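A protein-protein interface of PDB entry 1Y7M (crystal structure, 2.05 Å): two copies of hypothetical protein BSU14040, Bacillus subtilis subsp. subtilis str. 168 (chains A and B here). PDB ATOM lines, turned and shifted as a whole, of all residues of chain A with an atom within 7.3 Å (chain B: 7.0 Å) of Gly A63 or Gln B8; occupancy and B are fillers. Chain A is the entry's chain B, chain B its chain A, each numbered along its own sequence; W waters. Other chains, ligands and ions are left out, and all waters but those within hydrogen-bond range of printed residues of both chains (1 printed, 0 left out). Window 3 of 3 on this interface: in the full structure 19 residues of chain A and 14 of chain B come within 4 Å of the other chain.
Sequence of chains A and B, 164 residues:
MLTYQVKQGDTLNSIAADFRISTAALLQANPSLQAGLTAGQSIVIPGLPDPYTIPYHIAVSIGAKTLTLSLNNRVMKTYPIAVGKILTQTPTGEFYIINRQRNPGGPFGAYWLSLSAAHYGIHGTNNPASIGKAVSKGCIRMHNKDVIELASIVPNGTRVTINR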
ATOM      1  N   VAL A  60     -29.089 -14.449  -2.301  1.00  0.00           N
ATOM      2  CA  VAL A  60     -29.882 -15.654  -2.131  1.00  0.00           C
ATOM      3  C   VAL A  60     -29.039 -16.833  -2.530  1.00  0.00           C
ATOM      4  O   VAL A  60     -28.430 -16.824  -3.604  1.00  0.00           O
ATOM      5  CB  VAL A  60     -31.102 -15.568  -3.024  1.00  0.00           C
ATOM      6  CG1 VAL A  60     -31.825 -16.930  -3.125  1.00  0.00           C
ATOM      7  CG2 VAL A  60     -32.003 -14.476  -2.525  1.00  0.00           C
ATOM      8  N   SER A  61     -28.974 -17.834  -1.646  1.00  0.00           N
ATOM      9  CA  SER A  61     -28.333 -19.113  -1.950  1.00  0.00           C
ATOM     10  C   SER A  61     -29.415 -20.176  -2.090  1.00  0.00           C
ATOM     11  O   SER A  61     -30.106 -20.482  -1.121  1.00  0.00           O
ATOM     12  CB  SER A  61     -27.373 -19.510  -0.813  1.00  0.00           C
ATOM     13  OG  SER A  61     -26.730 -20.732  -1.095  1.00  0.00           O
ATOM     14  N   ILE A  62     -29.544 -20.751  -3.288  1.00  0.00           N
ATOM     15  CA  ILE A  62     -30.563 -21.756  -3.551  1.00  0.00           C
ATOM     16  C   ILE A  62     -30.254 -23.024  -2.770  1.00  0.00           C
ATOM     17  O   ILE A  62     -31.135 -23.579  -2.116  1.00  0.00           O
ATOM     18  CB  ILE A  62     -30.675 -22.029  -5.084  1.00  0.00           C
ATOM     19  CG1 ILE A  62     -31.287 -20.817  -5.779  1.00  0.00           C
ATOM     20  CG2 ILE A  62     -31.517 -23.294  -5.398  1.00  0.00           C
ATOM     21  CD1 ILE A  62     -31.148 -20.845  -7.273  1.00  0.00           C
ATOM     22  N   GLY A  63     -28.999 -23.463  -2.826  1.00  0.00           N
ATOM     23  CA  GLY A  63     -28.587 -24.708  -2.194  1.00  0.00           C
ATOM     24  C   GLY A  63     -28.835 -24.635  -0.703  1.00  0.00           C
ATOM     25  O   GLY A  63     -29.550 -25.471  -0.142  1.00  0.00           O
ATOM     26  N   ALA A  64     -28.269 -23.600  -0.075  1.00  0.00           N
ATOM     27  CA  ALA A  64     -28.416 -23.375   1.366  1.00  0.00           C
ATOM     28  C   ALA A  64     -29.809 -22.891   1.777  1.00  0.00           C
ATOM     29  O   ALA A  64     -30.109 -22.817   2.951  1.00  0.00           O
ATOM     30  CB  ALA A  64     -27.337 -22.399   1.864  1.00  0.00           C
ATOM     31  N   LYS A  65     -30.676 -22.572   0.815  1.00  0.00           N
ATOM     32  CA  LYS A  65     -32.023 -22.098   1.136  1.00  0.00           C
ATOM     33  C   LYS A  65     -32.001 -20.925   2.123  1.00  0.00           C
ATOM     34  O   LYS A  65     -32.757 -20.899   3.097  1.00  0.00           O
ATOM     35  CB  LYS A  65     -32.895 -23.217   1.704  1.00  0.00           C
ATOM     36  CG  LYS A  65     -32.814 -24.537   0.966  1.00  0.00           C
ATOM     37  CD  LYS A  65     -33.572 -24.546  -0.324  1.00  0.00           C
ATOM     38  CE  LYS A  65     -33.300 -25.829  -1.148  1.00  0.00           C
ATOM     39  NZ  LYS A  65     -32.588 -26.918  -0.417  1.00  0.00           N
ATOM     40  N   THR A  66     -31.118 -19.964   1.876  1.00  0.00           N
ATOM     41  CA  THR A  66     -31.085 -18.759   2.669  1.00  0.00           C
ATOM     42  C   THR A  66     -31.139 -17.499   1.830  1.00  0.00           C
ATOM     43  O   THR A  66     -30.634 -17.450   0.711  1.00  0.00           O
ATOM     44  CB  THR A  66     -29.826 -18.737   3.571  1.00  0.00           C
ATOM     45  OG1 THR A  66     -28.655 -18.924   2.773  1.00  0.00           O
ATOM     46  CG2 THR A  66     -29.822 -19.911   4.513  1.00  0.00           C
ATOM     47  N   VAL A  83     -37.452 -22.476  -2.292  1.00  0.00           N
ATOM     48  CA  VAL A  83     -36.993 -22.172  -3.647  1.00  0.00           C
ATOM     49  C   VAL A  83     -37.691 -23.083  -4.665  1.00  0.00           C
ATOM     50  O   VAL A  83     -38.442 -23.961  -4.290  1.00  0.00           O
ATOM     51  CB  VAL A  83     -35.476 -22.368  -3.762  1.00  0.00           C
ATOM     52  CG1 VAL A  83     -34.765 -21.532  -2.715  1.00  0.00           C
ATOM     53  CG2 VAL A  83     -35.103 -23.857  -3.643  1.00  0.00           C
ATOM     54  N   GLY A 132     -37.783 -23.680   3.532  1.00  0.00           N
ATOM     55  CA  GLY A 132     -36.605 -24.534   3.647  1.00  0.00           C
ATOM     56  C   GLY A 132     -36.563 -25.662   2.615  1.00  0.00           C
ATOM     57  O   GLY A 132     -35.659 -26.502   2.636  1.00  0.00           O
ATOM     58  N   ASN A 163     -27.621 -17.053  -6.335  1.00  0.00           N
ATOM     59  CA  ASN A 163     -26.563 -18.029  -6.613  1.00  0.00           C
ATOM     60  C   ASN A 163     -27.124 -19.426  -6.371  1.00  0.00           C
ATOM     61  O   ASN A 163     -28.083 -19.575  -5.642  1.00  0.00           O
ATOM     62  CB  ASN A 163     -25.407 -17.800  -5.620  1.00  0.00           C
ATOM     63  CG  ASN A 163     -24.855 -16.368  -5.665  1.00  0.00           C
ATOM     64  OD1 ASN A 163     -24.212 -15.984  -6.643  1.00  0.00           O
ATOM     65  ND2 ASN A 163     -25.116 -15.573  -4.614  1.00  0.00           N
ATOM     66  N   ARG A 164     -26.514 -20.430  -6.977  1.00  0.00           N
ATOM     67  CA  ARG A 164     -26.869 -21.819  -6.726  1.00  0.00           C
ATOM     68  C   ARG A 164     -26.551 -22.226  -5.292  1.00  0.00           C
ATOM     69  O   ARG A 164     -25.713 -21.619  -4.659  1.00  0.00           O
ATOM     70  CB  ARG A 164     -26.097 -22.727  -7.666  1.00  0.00           C
ATOM     71  N   GLN B   5     -20.588 -14.665  -1.550  1.00  0.00           N
ATOM     72  CA  GLN B   5     -21.500 -15.607  -0.906  1.00  0.00           C
ATOM     73  C   GLN B   5     -20.785 -16.928  -0.971  1.00  0.00           C
ATOM     74  O   GLN B   5     -20.515 -17.423  -2.074  1.00  0.00           O
ATOM     75  CB  GLN B   5     -22.866 -15.697  -1.624  1.00  0.00           C
ATOM     76  CG  GLN B   5     -23.837 -16.785  -1.056  1.00  0.00           C
ATOM     77  CD  GLN B   5     -25.257 -16.278  -0.774  1.00  0.00           C
ATOM     78  OE1 GLN B   5     -26.125 -16.367  -1.631  1.00  0.00           O
ATOM     79  NE2 GLN B   5     -25.492 -15.781   0.433  1.00  0.00           N
ATOM     80  N   VAL B   6     -20.433 -17.480   0.190  1.00  0.00           N
ATOM     81  CA  VAL B   6     -19.808 -18.802   0.217  1.00  0.00           C
ATOM     82  C   VAL B   6     -20.864 -19.813  -0.193  1.00  0.00           C
ATOM     83  O   VAL B   6     -21.946 -19.867   0.385  1.00  0.00           O
ATOM     84  CB  VAL B   6     -19.103 -19.189   1.582  1.00  0.00           C
ATOM     85  CG1 VAL B   6     -19.710 -18.512   2.773  1.00  0.00           C
ATOM     86  CG2 VAL B   6     -19.083 -20.717   1.792  1.00  0.00           C
ATOM     87  N   LYS B   7     -20.533 -20.594  -1.210  1.00  0.00           N
ATOM     88  CA  LYS B   7     -21.458 -21.534  -1.821  1.00  0.00           C
ATOM     89  C   LYS B   7     -21.282 -22.863  -1.107  1.00  0.00           C
ATOM     90  O   LYS B   7     -20.313 -23.049  -0.383  1.00  0.00           O
ATOM     91  CB  LYS B   7     -21.154 -21.716  -3.320  1.00  0.00           C
ATOM     92  CG  LYS B   7     -20.711 -20.454  -4.096  1.00  0.00           C
ATOM     93  CD  LYS B   7     -19.755 -20.817  -5.248  1.00  0.00           C
ATOM     94  CE  LYS B   7     -19.685 -19.772  -6.359  1.00  0.00           C
ATOM     95  NZ  LYS B   7     -18.280 -19.394  -6.705  1.00  0.00           N
ATOM     96  N   GLN B   8     -22.213 -23.782  -1.331  1.00  0.00           N
ATOM     97  CA  GLN B   8     -22.165 -25.101  -0.707  1.00  0.00           C
ATOM     98  C   GLN B   8     -21.013 -25.927  -1.287  1.00  0.00           C
ATOM     99  O   GLN B   8     -20.766 -25.889  -2.492  1.00  0.00           O
ATOM    100  CB  GLN B   8     -23.498 -25.826  -0.895  1.00  0.00           C
ATOM    101  CG  GLN B   8     -24.617 -25.303  -0.006  1.00  0.00           C
ATOM    102  CD  GLN B   8     -25.748 -26.295   0.131  1.00  0.00           C
ATOM    103  OE1 GLN B   8     -26.233 -26.826  -0.871  1.00  0.00           O
ATOM    104  NE2 GLN B   8     -26.168 -26.558   1.365  1.00  0.00           N
ATOM    105  N   GLY B   9     -20.300 -26.646  -0.421  1.00  0.00           N
ATOM    106  CA  GLY B   9     -19.092 -27.356  -0.819  1.00  0.00           C
ATOM    107  C   GLY B   9     -17.890 -26.463  -1.114  1.00  0.00           C
ATOM    108  O   GLY B   9     -16.927 -26.899  -1.755  1.00  0.00           O
ATOM    109  N   ASP B  10     -17.946 -25.206  -0.674  1.00  0.00           N
ATOM    110  CA  ASP B  10     -16.743 -24.390  -0.591  1.00  0.00           C
ATOM    111  C   ASP B  10     -16.105 -24.771   0.727  1.00  0.00           C
ATOM    112  O   ASP B  10     -16.796 -24.930   1.740  1.00  0.00           O
ATOM    113  CB  ASP B  10     -17.053 -22.888  -0.559  1.00  0.00           C
ATOM    114  CG  ASP B  10     -17.158 -22.256  -1.951  1.00  0.00           C
ATOM    115  OD1 ASP B  10     -16.950 -22.947  -2.964  1.00  0.00           O
ATOM    116  OD2 ASP B  10     -17.428 -21.051  -2.117  1.00  0.00           O
ATOM    117  N   THR B  11     -14.790 -24.941   0.707  1.00  0.00           N
ATOM    118  CA  THR B  11     -14.000 -24.909   1.932  1.00  0.00           C
ATOM    119  C   THR B  11     -13.335 -23.539   2.026  1.00  0.00           C
ATOM    120  O   THR B  11     -13.389 -22.745   1.074  1.00  0.00           O
ATOM    121  CB  THR B  11     -12.930 -25.987   1.912  1.00  0.00           C
ATOM    122  OG1 THR B  11     -11.932 -25.634   0.948  1.00  0.00           O
ATOM    123  CG2 THR B  11     -13.497 -27.340   1.421  1.00  0.00           C
ATOM    124  N   ALA B  39     -22.215 -22.068   4.691  1.00  0.00           N
ATOM    125  CA  ALA B  39     -22.795 -21.927   3.349  1.00  0.00           C
ATOM    126  C   ALA B  39     -24.031 -21.021   3.362  1.00  0.00           C
ATOM    127  O   ALA B  39     -24.987 -21.259   4.116  1.00  0.00           O
ATOM    128  CB  ALA B  39     -23.145 -23.294   2.756  1.00  0.00           C
ATOM    129  N   GLY B  40     -23.971 -19.967   2.549  1.00  0.00           N
ATOM    130  CA  GLY B  40     -25.065 -19.029   2.381  1.00  0.00           C
ATOM    131  C   GLY B  40     -24.812 -17.699   3.076  1.00  0.00           C
ATOM    132  O   GLY B  40     -25.517 -16.720   2.822  1.00  0.00           O
HETATM  133  O   HOH W   1     -27.871 -16.410   1.563  1.00  0.00           O
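The side-chain amide oxygen (OE1) of Gln B5 lies close to the backbone carbonyl oxygen (O) of Val A60 (3.1 Å). The side-chain amide oxygen (OE1) of Gln B5 is in hydrogen-bond range of the backbone NH (N) of Ser A61, 3.2 Å away. The side-chain amide oxygen of Gln B5 is in hydrogen-bond range of the side-chain amide nitrogen of Asn A163, at 3.2 Å.
The side-chain amide nitrogen (NE2) of Gln B5 is in hydrogen-bond range of the backbone carbonyl oxygen (O) of Gly B40 (2.6 Å). The backbone carbonyl oxygen of Val B6 sits at hydrogen-bond distance from the backbone NH of Gly B40 (3.0 Å). O of Val A60 is in hydrogen-bond range of N of Asn A163, 2.9 Å away. The side-chain hydroxyl (OG) of Ser A61 lies within hydrogen-bond range of the backbone NH (N) of Ala A64 (3.4 Å). N of Ser A61 lies within hydrogen-bond range of O of Thr A66 (2.9 Å). O of Asn A163 lies within hydrogen-bond range of N of Ile A62, at 3.0 Å.
CA of Gly B40 touches CB of Ser A61, 3.97 Å away. OE1 of Gln B8 touches C of Gly A63 (3.4 Å). CD of Gln B8 touches N of Ala A64 (3.7 Å). Ala A64 touches Ala B39 (CB to O, 3.4 Å). Thr A66 touches Gly B40.
Printed residues of chain B within 4 Å of Val A60: Gln B5 (3.1 Å). Printed residues of chain B within 4 Å of Ala A64: Gln B8 (3.7 Å) and Ala B39 (3.4 Å). Printed residues of chain B within 4 Å of Thr A66: Gly B40 (3.6 Å). Val A83 touches none of the printed residues of chain B. Of the printed residues of chain B, Asn A163 touches Gln B5. Lys B7 touches none of the printed residues of chain A. Gln B8 touches just these residues of chain A: Gly A63 and Ala A64. Of the printed residues of chain A, Gly B40 touches Ser A61 and Thr A66.
Of the 9 printed residues of chain B, 4 touch a printed residue of chain A. Along chain B the printed residues that touch a printed residue of chain A span positions 5 to 40. Printed residues of chain A that touch a printed residue of chain B: Val A60, Ser A61, Gly A63, Ala A64, Thr A66 and Asn A163. Hydrophobic or aromatic side chains of chain A within 4 Å of the printed part of chain B: Ala A64. Among the printed residues, 8 pairs touch across the chains. Among the printed residues, no Asp or Glu carboxylate lies within 4 Å of a Lys or Arg side-chain nitrogen of the other chain.
No position is printed for both chains. Of the 8 pairs that touch across the chains among the printed residues, none has its exchanged pair printed and touching as well.
Water W1 lies within hydrogen-bond range of O of Gly B40 (2.7 Å), NE2 of Gln B5 (2.7 Å) and OG1 of Thr A66 (2.9 Å).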
